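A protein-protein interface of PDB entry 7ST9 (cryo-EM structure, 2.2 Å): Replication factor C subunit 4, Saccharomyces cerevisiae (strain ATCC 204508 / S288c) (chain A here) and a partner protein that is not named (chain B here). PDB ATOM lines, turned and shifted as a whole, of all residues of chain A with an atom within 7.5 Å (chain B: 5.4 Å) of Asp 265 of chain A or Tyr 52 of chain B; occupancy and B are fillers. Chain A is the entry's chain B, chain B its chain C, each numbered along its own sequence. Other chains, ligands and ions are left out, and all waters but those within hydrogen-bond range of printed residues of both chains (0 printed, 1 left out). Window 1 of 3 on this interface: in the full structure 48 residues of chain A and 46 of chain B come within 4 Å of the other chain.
Hydrophobic or aromatic side chains of chain B within 4 Å of the printed part of chain A: Tyr 52, Pro 54, Tyr 149, Ala 150 and His 151.
Among the printed residues, 15 pairs touch across the chains.
The backbone carbonyl oxygen of Leu 256 of chain A sits at hydrogen-bond distance from the backbone NH of Tyr 261 of chain A.
The side-chain carboxylate of Asp 265 of chain A sits at hydrogen-bond distance from the side-chain hydroxyl of Ser 262 of chain A (2.8 Å).
The backbone carbonyl oxygen (O) of Ile 264 of chain A sits at hydrogen-bond distance from the side-chain hydroxyl (OG1) of Thr 268 of chain A, at 2.9 Å.
O of Phe 164 of chain B sits at hydrogen-bond distance from N of Tyr 52 of chain B (3.0 Å).
The backbone carbonyl oxygen of Tyr 52 of chain B is in hydrogen-bond range of the backbone NH of Phe 166 of chain B (2.9 Å).
ND2 of Asn 148 of chain B is in hydrogen-bond range of O of Gly 53 of chain B (2.6 Å).
Gly 260 of chain A touches Pro 54 of chain B.
OH of Tyr 52 of chain B touches CA of Tyr 261 of chain A (3.6 Å).
Ser 262 of chain A touches Asn 148 of chain B.
Ser 262 of chain A touches Tyr 149 of chain B (OG to CD1, 3.6 Å).
Ile 264 of chain A touches Tyr 149 of chain B (CG2 to CD1, 3.6 Å).
NE2 of His 151 of chain B touches CG1 of Ile 264 of chain A, at 3.3 Å.
Asp 265 of chain A touches Asn 148 of chain B.
Tyr 149 of chain B touches Asp 265 of chain A (CA to OD2, 3.3 Å).
CB of His 151 of chain B touches OG1 of Thr 268 of chain A, at 3.8 Å.
NH1 of Arg 165 of chain B sits at hydrogen-bond distance from O of Lys 259 of chain A (3.0 Å).
OH of Tyr 261 of chain A is in hydrogen-bond range of NH2 of Arg 163 of chain B, at 3.1 Å.
The backbone NH (N) of Ser 262 of chain A sits at hydrogen-bond distance from the side-chain hydroxyl (OH) of Tyr 52 of chain B (3.2 Å).
The side-chain hydroxyl (OH) of Tyr 52 of chain B sits at hydrogen-bond distance from the side-chain carboxylate (OD2) of Asp 265 of chain A, at 2.7 Å.
OD2 of Asp 265 of chain A is in hydrogen-bond range of N of Ala 150 of chain B.
N of His 151 of chain B is in hydrogen-bond range of OD1 of Asp 265 of chain A.
Of the printed residues of chain B, Ser 262 of chain A touches Tyr 52 (3.2 Å), Asn 148 (3.7 Å) and Tyr 149 (3.6 Å).
Of chain B, only Tyr 52, Asn 148, Tyr 149, Ala 150 and His 151 come within 4 Å of Asp 265 of chain A.
Tyr 52 of chain B touches three residues of chain A.
Of the printed residues of chain A, Pro 54 of chain B touches Gly 260 (3.8 Å).
The nearest residue of chain B that does not touch Asp 265 of chain A is Lys 152 of chain B (4.9 Å).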
ATOM      1  N   HIS A 232      14.110   0.370  20.300  1.00  0.00           N
ATOM      2  CA  HIS A 232      13.488  -0.928  20.079  1.00  0.00           C
ATOM      3  C   HIS A 232      13.840  -1.949  21.161  1.00  0.00           C
ATOM      4  O   HIS A 232      13.079  -2.905  21.348  1.00  0.00           O
ATOM      5  CB  HIS A 232      13.848  -1.474  18.691  1.00  0.00           C
ATOM      6  CG  HIS A 232      15.313  -1.685  18.471  1.00  0.00           C
ATOM      7  ND1 HIS A 232      15.938  -2.886  18.723  1.00  0.00           N
ATOM      8  CD2 HIS A 232      16.272  -0.852  18.002  1.00  0.00           C
ATOM      9  CE1 HIS A 232      17.222  -2.783  18.430  1.00  0.00           C
ATOM     10  NE2 HIS A 232      17.451  -1.558  17.992  1.00  0.00           N
ATOM     11  N   VAL A 236      11.195  -4.651  22.646  1.00  0.00           N
ATOM     12  CA  VAL A 236      11.458  -6.084  22.716  1.00  0.00           C
ATOM     13  C   VAL A 236      11.257  -6.593  24.137  1.00  0.00           C
ATOM     14  O   VAL A 236      10.721  -7.685  24.353  1.00  0.00           O
ATOM     15  CB  VAL A 236      12.877  -6.386  22.197  1.00  0.00           C
ATOM     16  CG1 VAL A 236      13.277  -7.815  22.522  1.00  0.00           C
ATOM     17  CG2 VAL A 236      12.958  -6.133  20.698  1.00  0.00           C
ATOM     18  N   LEU A 256       7.097  -3.730  15.760  1.00  0.00           N
ATOM     19  CA  LEU A 256       8.381  -4.148  15.206  1.00  0.00           C
ATOM     20  C   LEU A 256       8.286  -4.533  13.735  1.00  0.00           C
ATOM     21  O   LEU A 256       8.995  -3.952  12.908  1.00  0.00           O
ATOM     22  CB  LEU A 256       8.944  -5.312  16.032  1.00  0.00           C
ATOM     23  CG  LEU A 256       9.252  -4.992  17.497  1.00  0.00           C
ATOM     24  CD1 LEU A 256       9.514  -6.268  18.284  1.00  0.00           C
ATOM     25  CD2 LEU A 256      10.434  -4.040  17.608  1.00  0.00           C
ATOM     26  N   LYS A 259       6.982  -1.885  11.192  1.00  0.00           N
ATOM     27  CA  LYS A 259       7.846  -0.714  11.120  1.00  0.00           C
ATOM     28  C   LYS A 259       9.124  -0.968  10.332  1.00  0.00           C
ATOM     29  O   LYS A 259       9.944  -0.054  10.202  1.00  0.00           O
ATOM     30  CB  LYS A 259       8.196  -0.232  12.530  1.00  0.00           C
ATOM     31  CG  LYS A 259       6.991   0.223  13.336  1.00  0.00           C
ATOM     32  CD  LYS A 259       7.301   1.469  14.146  1.00  0.00           C
ATOM     33  CE  LYS A 259       6.136   1.851  15.046  1.00  0.00           C
ATOM     34  NZ  LYS A 259       4.919   2.206  14.268  1.00  0.00           N
ATOM     35  N   GLY A 260       9.314  -2.174   9.805  1.00  0.00           N
ATOM     36  CA  GLY A 260      10.452  -2.469   8.962  1.00  0.00           C
ATOM     37  C   GLY A 260      11.661  -3.041   9.667  1.00  0.00           C
ATOM     38  O   GLY A 260      12.717  -3.171   9.037  1.00  0.00           O
ATOM     39  N   TYR A 261      11.550  -3.387  10.947  1.00  0.00           N
ATOM     40  CA  TYR A 261      12.673  -3.988  11.652  1.00  0.00           C
ATOM     41  C   TYR A 261      12.913  -5.403  11.137  1.00  0.00           C
ATOM     42  O   TYR A 261      11.980  -6.206  11.035  1.00  0.00           O
ATOM     43  CB  TYR A 261      12.406  -4.007  13.157  1.00  0.00           C
ATOM     44  CG  TYR A 261      12.573  -2.658  13.819  1.00  0.00           C
ATOM     45  CD1 TYR A 261      13.833  -2.172  14.142  1.00  0.00           C
ATOM     46  CD2 TYR A 261      11.471  -1.869  14.119  1.00  0.00           C
ATOM     47  CE1 TYR A 261      13.989  -0.940  14.746  1.00  0.00           C
ATOM     48  CE2 TYR A 261      11.617  -0.636  14.723  1.00  0.00           C
ATOM     49  CZ  TYR A 261      12.879  -0.177  15.033  1.00  0.00           C
ATOM     50  OH  TYR A 261      13.030   1.051  15.635  1.00  0.00           O
ATOM     51  N   SER A 262      14.166  -5.706  10.809  1.00  0.00           N
ATOM     52  CA  SER A 262      14.509  -7.018  10.280  1.00  0.00           C
ATOM     53  C   SER A 262      14.430  -8.079  11.374  1.00  0.00           C
ATOM     54  O   SER A 262      14.623  -7.801  12.560  1.00  0.00           O
ATOM     55  CB  SER A 262      15.910  -6.997   9.671  1.00  0.00           C
ATOM     56  OG  SER A 262      16.903  -6.868  10.671  1.00  0.00           O
ATOM     57  N   SER A 263      14.140  -9.314  10.956  1.00  0.00           N
ATOM     58  CA  SER A 263      14.000 -10.408  11.913  1.00  0.00           C
ATOM     59  C   SER A 263      15.310 -10.676  12.646  1.00  0.00           C
ATOM     60  O   SER A 263      15.309 -10.967  13.848  1.00  0.00           O
ATOM     61  CB  SER A 263      13.517 -11.669  11.196  1.00  0.00           C
ATOM     62  OG  SER A 263      14.502 -12.164  10.306  1.00  0.00           O
ATOM     63  N   ILE A 264      16.438 -10.589  11.937  1.00  0.00           N
ATOM     64  CA  ILE A 264      17.733 -10.830  12.569  1.00  0.00           C
ATOM     65  C   ILE A 264      17.977  -9.816  13.681  1.00  0.00           C
ATOM     66  O   ILE A 264      18.426 -10.170  14.782  1.00  0.00           O
ATOM     67  CB  ILE A 264      18.855 -10.808  11.510  1.00  0.00           C
ATOM     68  CG1 ILE A 264      20.191 -11.232  12.127  1.00  0.00           C
ATOM     69  CG2 ILE A 264      18.978  -9.430  10.867  1.00  0.00           C
ATOM     70  CD1 ILE A 264      20.253 -12.692  12.513  1.00  0.00           C
ATOM     71  N   ASP A 265      17.681  -8.540  13.418  1.00  0.00           N
ATOM     72  CA  ASP A 265      17.814  -7.523  14.454  1.00  0.00           C
ATOM     73  C   ASP A 265      16.903  -7.830  15.634  1.00  0.00           C
ATOM     74  O   ASP A 265      17.300  -7.674  16.795  1.00  0.00           O
ATOM     75  CB  ASP A 265      17.494  -6.140  13.881  1.00  0.00           C
ATOM     76  CG  ASP A 265      18.572  -5.628  12.943  1.00  0.00           C
ATOM     77  OD1 ASP A 265      19.752  -5.989  13.129  1.00  0.00           O
ATOM     78  OD2 ASP A 265      18.239  -4.861  12.016  1.00  0.00           O
ATOM     79  N   ILE A 266      15.677  -8.275  15.355  1.00  0.00           N
ATOM     80  CA  ILE A 266      14.726  -8.567  16.425  1.00  0.00           C
ATOM     81  C   ILE A 266      15.259  -9.678  17.321  1.00  0.00           C
ATOM     82  O   ILE A 266      15.205  -9.582  18.550  1.00  0.00           O
ATOM     83  CB  ILE A 266      13.351  -8.924  15.835  1.00  0.00           C
ATOM     84  CG1 ILE A 266      12.683  -7.674  15.257  1.00  0.00           C
ATOM     85  CG2 ILE A 266      12.462  -9.559  16.898  1.00  0.00           C
ATOM     86  CD1 ILE A 266      11.546  -7.969  14.305  1.00  0.00           C
ATOM     87  N   VAL A 267      15.787 -10.748  16.722  1.00  0.00           N
ATOM     88  CA  VAL A 267      16.250 -11.877  17.528  1.00  0.00           C
ATOM     89  C   VAL A 267      17.511 -11.507  18.303  1.00  0.00           C
ATOM     90  O   VAL A 267      17.676 -11.901  19.467  1.00  0.00           O
ATOM     91  CB  VAL A 267      16.463 -13.128  16.656  1.00  0.00           C
ATOM     92  CG1 VAL A 267      15.135 -13.604  16.086  1.00  0.00           C
ATOM     93  CG2 VAL A 267      17.466 -12.865  15.545  1.00  0.00           C
ATOM     94  N   THR A 268      18.424 -10.753  17.684  1.00  0.00           N
ATOM     95  CA  THR A 268      19.616 -10.328  18.413  1.00  0.00           C
ATOM     96  C   THR A 268      19.244  -9.450  19.604  1.00  0.00           C
ATOM     97  O   THR A 268      19.768  -9.632  20.714  1.00  0.00           O
ATOM     98  CB  THR A 268      20.574  -9.586  17.477  1.00  0.00           C
ATOM     99  OG1 THR A 268      19.857  -8.584  16.744  1.00  0.00           O
ATOM    100  CG2 THR A 268      21.225 -10.555  16.503  1.00  0.00           C
ATOM    101  N   THR A 269      18.323  -8.504  19.398  1.00  0.00           N
ATOM    102  CA  THR A 269      17.872  -7.661  20.498  1.00  0.00           C
ATOM    103  C   THR A 269      17.164  -8.486  21.565  1.00  0.00           C
ATOM    104  O   THR A 269      17.293  -8.206  22.761  1.00  0.00           O
ATOM    105  CB  THR A 269      16.951  -6.560  19.973  1.00  0.00           C
ATOM    106  OG1 THR A 269      17.640  -5.790  18.982  1.00  0.00           O
ATOM    107  CG2 THR A 269      16.508  -5.645  21.105  1.00  0.00           C
ATOM    108  N   SER A 270      16.398  -9.498  21.153  1.00  0.00           N
ATOM    109  CA  SER A 270      15.727 -10.357  22.121  1.00  0.00           C
ATOM    110  C   SER A 270      16.737 -11.082  22.997  1.00  0.00           C
ATOM    111  O   SER A 270      16.563 -11.168  24.217  1.00  0.00           O
ATOM    112  CB  SER A 270      14.828 -11.361  21.401  1.00  0.00           C
ATOM    113  OG  SER A 270      13.737 -10.713  20.772  1.00  0.00           O
ATOM    114  N   PHE A 271      17.801 -11.611  22.392  1.00  0.00           N
ATOM    115  CA  PHE A 271      18.839 -12.271  23.178  1.00  0.00           C
ATOM    116  C   PHE A 271      19.485 -11.293  24.153  1.00  0.00           C
ATOM    117  O   PHE A 271      19.653 -11.595  25.344  1.00  0.00           O
ATOM    118  CB  PHE A 271      19.889 -12.883  22.250  1.00  0.00           C
ATOM    119  CG  PHE A 271      21.063 -13.485  22.971  1.00  0.00           C
ATOM    120  CD1 PHE A 271      20.870 -14.365  24.023  1.00  0.00           C
ATOM    121  CD2 PHE A 271      22.357 -13.174  22.594  1.00  0.00           C
ATOM    122  CE1 PHE A 271      21.948 -14.921  24.686  1.00  0.00           C
ATOM    123  CE2 PHE A 271      23.440 -13.728  23.253  1.00  0.00           C
ATOM    124  CZ  PHE A 271      23.234 -14.603  24.300  1.00  0.00           C
ATOM    125  N   ARG A 272      19.840 -10.100  23.664  1.00  0.00           N
ATOM    126  CA  ARG A 272      20.483  -9.118  24.532  1.00  0.00           C
ATOM    127  C   ARG A 272      19.579  -8.734  25.698  1.00  0.00           C
ATOM    128  O   ARG A 272      20.037  -8.628  26.841  1.00  0.00           O
ATOM    129  CB  ARG A 272      20.874  -7.878  23.727  1.00  0.00           C
ATOM    130  CG  ARG A 272      21.950  -8.132  22.682  1.00  0.00           C
ATOM    131  CD  ARG A 272      22.651  -6.846  22.264  1.00  0.00           C
ATOM    132  NE  ARG A 272      21.858  -6.065  21.320  1.00  0.00           N
ATOM    133  CZ  ARG A 272      21.011  -5.102  21.657  1.00  0.00           C
ATOM    134  NH1 ARG A 272      20.808  -4.768  22.922  1.00  0.00           N
ATOM    135  NH2 ARG A 272      20.349  -4.456  20.702  1.00  0.00           N
ATOM    136  N   ILE A 299      16.899 -18.455  11.308  1.00  0.00           N
ATOM    137  CA  ILE A 299      16.929 -17.226  10.518  1.00  0.00           C
ATOM    138  C   ILE A 299      18.202 -17.155   9.684  1.00  0.00           C
ATOM    139  O   ILE A 299      18.171 -16.765   8.511  1.00  0.00           O
ATOM    140  CB  ILE A 299      16.789 -15.996  11.436  1.00  0.00           C
ATOM    141  CG1 ILE A 299      15.346 -15.865  11.926  1.00  0.00           C
ATOM    142  CG2 ILE A 299      17.221 -14.729  10.705  1.00  0.00           C
ATOM    143  CD1 ILE A 299      15.186 -14.927  13.098  1.00  0.00           C
ATOM    144  N   LEU A 309       9.314 -15.959  14.167  1.00  0.00           N
ATOM    145  CA  LEU A 309       9.301 -15.121  15.363  1.00  0.00           C
ATOM    146  C   LEU A 309       8.062 -15.391  16.211  1.00  0.00           C
ATOM    147  O   LEU A 309       8.140 -15.422  17.446  1.00  0.00           O
ATOM    148  CB  LEU A 309       9.375 -13.646  14.969  1.00  0.00           C
ATOM    149  CG  LEU A 309      10.671 -13.212  14.280  1.00  0.00           C
ATOM    150  CD1 LEU A 309      10.524 -11.827  13.670  1.00  0.00           C
ATOM    151  CD2 LEU A 309      11.838 -13.244  15.254  1.00  0.00           C
ATOM    152  N   LEU B  50      21.842   8.211   8.541  1.00  0.00           N
ATOM    153  CA  LEU B  50      21.669   6.768   8.461  1.00  0.00           C
ATOM    154  C   LEU B  50      20.258   6.504   7.963  1.00  0.00           C
ATOM    155  O   LEU B  50      19.299   7.065   8.494  1.00  0.00           O
ATOM    156  CB  LEU B  50      21.894   6.096   9.824  1.00  0.00           C
ATOM    157  CG  LEU B  50      21.348   4.674   9.995  1.00  0.00           C
ATOM    158  CD1 LEU B  50      22.054   3.707   9.059  1.00  0.00           C
ATOM    159  CD2 LEU B  50      21.488   4.215  11.437  1.00  0.00           C
ATOM    160  N   PHE B  51      20.140   5.675   6.931  1.00  0.00           N
ATOM    161  CA  PHE B  51      18.856   5.258   6.378  1.00  0.00           C
ATOM    162  C   PHE B  51      18.709   3.767   6.644  1.00  0.00           C
ATOM    163  O   PHE B  51      19.376   2.948   6.001  1.00  0.00           O
ATOM    164  CB  PHE B  51      18.772   5.556   4.880  1.00  0.00           C
ATOM    165  CG  PHE B  51      18.585   7.016   4.543  1.00  0.00           C
ATOM    166  CD1 PHE B  51      18.429   7.974   5.534  1.00  0.00           C
ATOM    167  CD2 PHE B  51      18.563   7.425   3.219  1.00  0.00           C
ATOM    168  CE1 PHE B  51      18.256   9.307   5.209  1.00  0.00           C
ATOM    169  CE2 PHE B  51      18.392   8.757   2.890  1.00  0.00           C
ATOM    170  CZ  PHE B  51      18.239   9.698   3.885  1.00  0.00           C
ATOM    171  N   TYR B  52      17.840   3.415   7.586  1.00  0.00           N
ATOM    172  CA  TYR B  52      17.621   2.028   7.968  1.00  0.00           C
ATOM    173  C   TYR B  52      16.255   1.582   7.474  1.00  0.00           C
ATOM    174  O   TYR B  52      15.253   2.262   7.720  1.00  0.00           O
ATOM    175  CB  TYR B  52      17.717   1.853   9.485  1.00  0.00           C
ATOM    176  CG  TYR B  52      17.315   0.476   9.962  1.00  0.00           C
ATOM    177  CD1 TYR B  52      18.193  -0.595   9.871  1.00  0.00           C
ATOM    178  CD2 TYR B  52      16.054   0.247  10.499  1.00  0.00           C
ATOM    179  CE1 TYR B  52      17.830  -1.856  10.306  1.00  0.00           C
ATOM    180  CE2 TYR B  52      15.682  -1.011  10.935  1.00  0.00           C
ATOM    181  CZ  TYR B  52      16.573  -2.059  10.836  1.00  0.00           C
ATOM    182  OH  TYR B  52      16.208  -3.312  11.268  1.00  0.00           O
ATOM    183  N   GLY B  53      16.209   0.447   6.781  1.00  0.00           N
ATOM    184  CA  GLY B  53      14.940  -0.065   6.316  1.00  0.00           C
ATOM    185  C   GLY B  53      15.013  -1.359   5.531  1.00  0.00           C
ATOM    186  O   GLY B  53      16.087  -1.831   5.148  1.00  0.00           O
ATOM    187  N   PRO B  54      13.849  -1.949   5.271  1.00  0.00           N
ATOM    188  CA  PRO B  54      13.800  -3.219   4.542  1.00  0.00           C
ATOM    189  C   PRO B  54      13.966  -3.006   3.048  1.00  0.00           C
ATOM    190  O   PRO B  54      13.951  -1.863   2.569  1.00  0.00           O
ATOM    191  CB  PRO B  54      12.404  -3.762   4.880  1.00  0.00           C
ATOM    192  CG  PRO B  54      11.586  -2.551   5.146  1.00  0.00           C
ATOM    193  CD  PRO B  54      12.511  -1.492   5.682  1.00  0.00           C
ATOM    194  N   LYS B  59      15.655   3.862  -0.148  1.00  0.00           N
ATOM    195  CA  LYS B  59      16.811   4.463   0.510  1.00  0.00           C
ATOM    196  C   LYS B  59      17.840   4.931  -0.513  1.00  0.00           C
ATOM    197  O   LYS B  59      18.246   6.102  -0.512  1.00  0.00           O
ATOM    198  CB  LYS B  59      17.432   3.463   1.487  1.00  0.00           C
ATOM    199  CG  LYS B  59      16.445   2.901   2.503  1.00  0.00           C
ATOM    200  CD  LYS B  59      17.124   1.988   3.517  1.00  0.00           C
ATOM    201  CE  LYS B  59      17.539   0.656   2.903  1.00  0.00           C
ATOM    202  NZ  LYS B  59      16.378  -0.143   2.418  1.00  0.00           N
ATOM    203  N   ALA B 147      21.347   0.876   5.394  1.00  0.00           N
ATOM    204  CA  ALA B 147      21.386  -0.455   5.981  1.00  0.00           C
ATOM    205  C   ALA B 147      19.999  -1.081   6.033  1.00  0.00           C
ATOM    206  O   ALA B 147      18.977  -0.388   6.117  1.00  0.00           O
ATOM    207  CB  ALA B 147      21.987  -0.417   7.391  1.00  0.00           C
ATOM    208  N   ASN B 148      19.990  -2.416   5.979  1.00  0.00           N
ATOM    209  CA  ASN B 148      18.815  -3.219   6.278  1.00  0.00           C
ATOM    210  C   ASN B 148      18.906  -3.928   7.621  1.00  0.00           C
ATOM    211  O   ASN B 148      17.866  -4.281   8.185  1.00  0.00           O
ATOM    212  CB  ASN B 148      18.591  -4.275   5.184  1.00  0.00           C
ATOM    213  CG  ASN B 148      18.629  -3.690   3.784  1.00  0.00           C
ATOM    214  OD1 ASN B 148      19.643  -3.775   3.092  1.00  0.00           O
ATOM    215  ND2 ASN B 148      17.520  -3.099   3.360  1.00  0.00           N
ATOM    216  N   TYR B 149      20.114  -4.144   8.142  1.00  0.00           N
ATOM    217  CA  TYR B 149      20.328  -4.858   9.398  1.00  0.00           C
ATOM    218  C   TYR B 149      21.198  -3.995  10.301  1.00  0.00           C
ATOM    219  O   TYR B 149      22.392  -3.821  10.037  1.00  0.00           O
ATOM    220  CB  TYR B 149      20.980  -6.218   9.149  1.00  0.00           C
ATOM    221  CG  TYR B 149      20.422  -6.944   7.945  1.00  0.00           C
ATOM    222  CD1 TYR B 149      19.108  -7.389   7.927  1.00  0.00           C
ATOM    223  CD2 TYR B 149      21.208  -7.176   6.824  1.00  0.00           C
ATOM    224  CE1 TYR B 149      18.593  -8.050   6.829  1.00  0.00           C
ATOM    225  CE2 TYR B 149      20.702  -7.836   5.721  1.00  0.00           C
ATOM    226  CZ  TYR B 149      19.394  -8.270   5.729  1.00  0.00           C
ATOM    227  OH  TYR B 149      18.883  -8.928   4.634  1.00  0.00           O
ATOM    228  N   ALA B 150      20.602  -3.461  11.369  1.00  0.00           N
ATOM    229  CA  ALA B 150      21.337  -2.562  12.254  1.00  0.00           C
ATOM    230  C   ALA B 150      22.325  -3.312  13.139  1.00  0.00           C
ATOM    231  O   ALA B 150      23.339  -2.739  13.551  1.00  0.00           O
ATOM    232  CB  ALA B 150      20.359  -1.764  13.116  1.00  0.00           C
ATOM    233  N   HIS B 151      22.055  -4.584  13.440  1.00  0.00           N
ATOM    234  CA  HIS B 151      22.931  -5.332  14.335  1.00  0.00           C
ATOM    235  C   HIS B 151      24.340  -5.478  13.776  1.00  0.00           C
ATOM    236  O   HIS B 151      25.270  -5.757  14.539  1.00  0.00           O
ATOM    237  CB  HIS B 151      22.339  -6.716  14.621  1.00  0.00           C
ATOM    238  CG  HIS B 151      22.569  -7.711  13.528  1.00  0.00           C
ATOM    239  ND1 HIS B 151      23.547  -8.679  13.596  1.00  0.00           N
ATOM    240  CD2 HIS B 151      21.946  -7.890  12.338  1.00  0.00           C
ATOM    241  CE1 HIS B 151      23.518  -9.410  12.497  1.00  0.00           C
ATOM    242  NE2 HIS B 151      22.556  -8.951  11.717  1.00  0.00           N
ATOM    243  N   LYS B 152      24.521  -5.297  12.467  1.00  0.00           N
ATOM    244  CA  LYS B 152      25.848  -5.361  11.869  1.00  0.00           C
ATOM    245  C   LYS B 152      26.637  -4.067  12.032  1.00  0.00           C
ATOM    246  O   LYS B 152      27.850  -4.070  11.796  1.00  0.00           O
ATOM    247  CB  LYS B 152      25.737  -5.702  10.379  1.00  0.00           C
ATOM    248  CG  LYS B 152      25.204  -7.100  10.093  1.00  0.00           C
ATOM    249  CD  LYS B 152      26.202  -8.192  10.467  1.00  0.00           C
ATOM    250  CE  LYS B 152      27.439  -8.179   9.576  1.00  0.00           C
ATOM    251  NZ  LYS B 152      27.106  -8.194   8.124  1.00  0.00           N
ATOM    252  N   ARG B 163      19.500   9.049  12.631  1.00  0.00           N
ATOM    253  CA  ARG B 163      18.809   7.880  12.105  1.00  0.00           C
ATOM    254  C   ARG B 163      17.471   8.258  11.485  1.00  0.00           C
ATOM    255  O   ARG B 163      16.714   9.059  12.042  1.00  0.00           O
ATOM    256  CB  ARG B 163      18.595   6.849  13.215  1.00  0.00           C
ATOM    257  CG  ARG B 163      17.542   5.796  12.905  1.00  0.00           C
ATOM    258  CD  ARG B 163      17.701   4.585  13.811  1.00  0.00           C
ATOM    259  NE  ARG B 163      16.763   3.517  13.486  1.00  0.00           N
ATOM    260  CZ  ARG B 163      15.478   3.520  13.811  1.00  0.00           C
ATOM    261  NH1 ARG B 163      14.931   4.537  14.458  1.00  0.00           N
ATOM    262  NH2 ARG B 163      14.722   2.478  13.481  1.00  0.00           N
ATOM    263  N   PHE B 164      17.183   7.667  10.326  1.00  0.00           N
ATOM    264  CA  PHE B 164      15.897   7.794   9.656  1.00  0.00           C
ATOM    265  C   PHE B 164      15.444   6.406   9.230  1.00  0.00           C
ATOM    266  O   PHE B 164      16.201   5.670   8.582  1.00  0.00           O
ATOM    267  CB  PHE B 164      15.984   8.725   8.441  1.00  0.00           C
ATOM    268  CG  PHE B 164      16.201  10.169   8.796  1.00  0.00           C
ATOM    269  CD1 PHE B 164      15.137  10.973   9.170  1.00  0.00           C
ATOM    270  CD2 PHE B 164      17.467  10.726   8.750  1.00  0.00           C
ATOM    271  CE1 PHE B 164      15.332  12.301   9.494  1.00  0.00           C
ATOM    272  CE2 PHE B 164      17.668  12.054   9.074  1.00  0.00           C
ATOM    273  CZ  PHE B 164      16.599  12.842   9.446  1.00  0.00           C
ATOM    274  N   ARG B 165      14.211   6.061   9.584  1.00  0.00           N
ATOM    275  CA  ARG B 165      13.650   4.744   9.319  1.00  0.00           C
ATOM    276  C   ARG B 165      12.741   4.822   8.100  1.00  0.00           C
ATOM    277  O   ARG B 165      11.797   5.618   8.073  1.00  0.00           O
ATOM    278  CB  ARG B 165      12.874   4.233  10.532  1.00  0.00           C
ATOM    279  CG  ARG B 165      12.483   2.766  10.445  1.00  0.00           C
ATOM    280  CD  ARG B 165      11.714   2.303  11.676  1.00  0.00           C
ATOM    281  NE  ARG B 165      10.782   3.312  12.165  1.00  0.00           N
ATOM    282  CZ  ARG B 165       9.569   3.521  11.668  1.00  0.00           C
ATOM    283  NH1 ARG B 165       9.102   2.804  10.660  1.00  0.00           N
ATOM    284  NH2 ARG B 165       8.808   4.475  12.195  1.00  0.00           N
ATOM    285  N   PHE B 166      13.029   3.997   7.098  1.00  0.00           N
ATOM    286  CA  PHE B 166      12.171   3.856   5.928  1.00  0.00           C
ATOM    287  C   PHE B 166      11.178   2.735   6.208  1.00  0.00           C
ATOM    288  O   PHE B 166      11.548   1.556   6.223  1.00  0.00           O
ATOM    289  CB  PHE B 166      12.998   3.566   4.679  1.00  0.00           C
ATOM    290  CG  PHE B 166      13.654   4.784   4.091  1.00  0.00           C
ATOM    291  CD1 PHE B 166      14.613   5.482   4.804  1.00  0.00           C
ATOM    292  CD2 PHE B 166      13.309   5.229   2.826  1.00  0.00           C
ATOM    293  CE1 PHE B 166      15.218   6.602   4.266  1.00  0.00           C
ATOM    294  CE2 PHE B 166      13.910   6.348   2.283  1.00  0.00           C
ATOM    295  CZ  PHE B 166      14.866   7.035   3.003  1.00  0.00           C
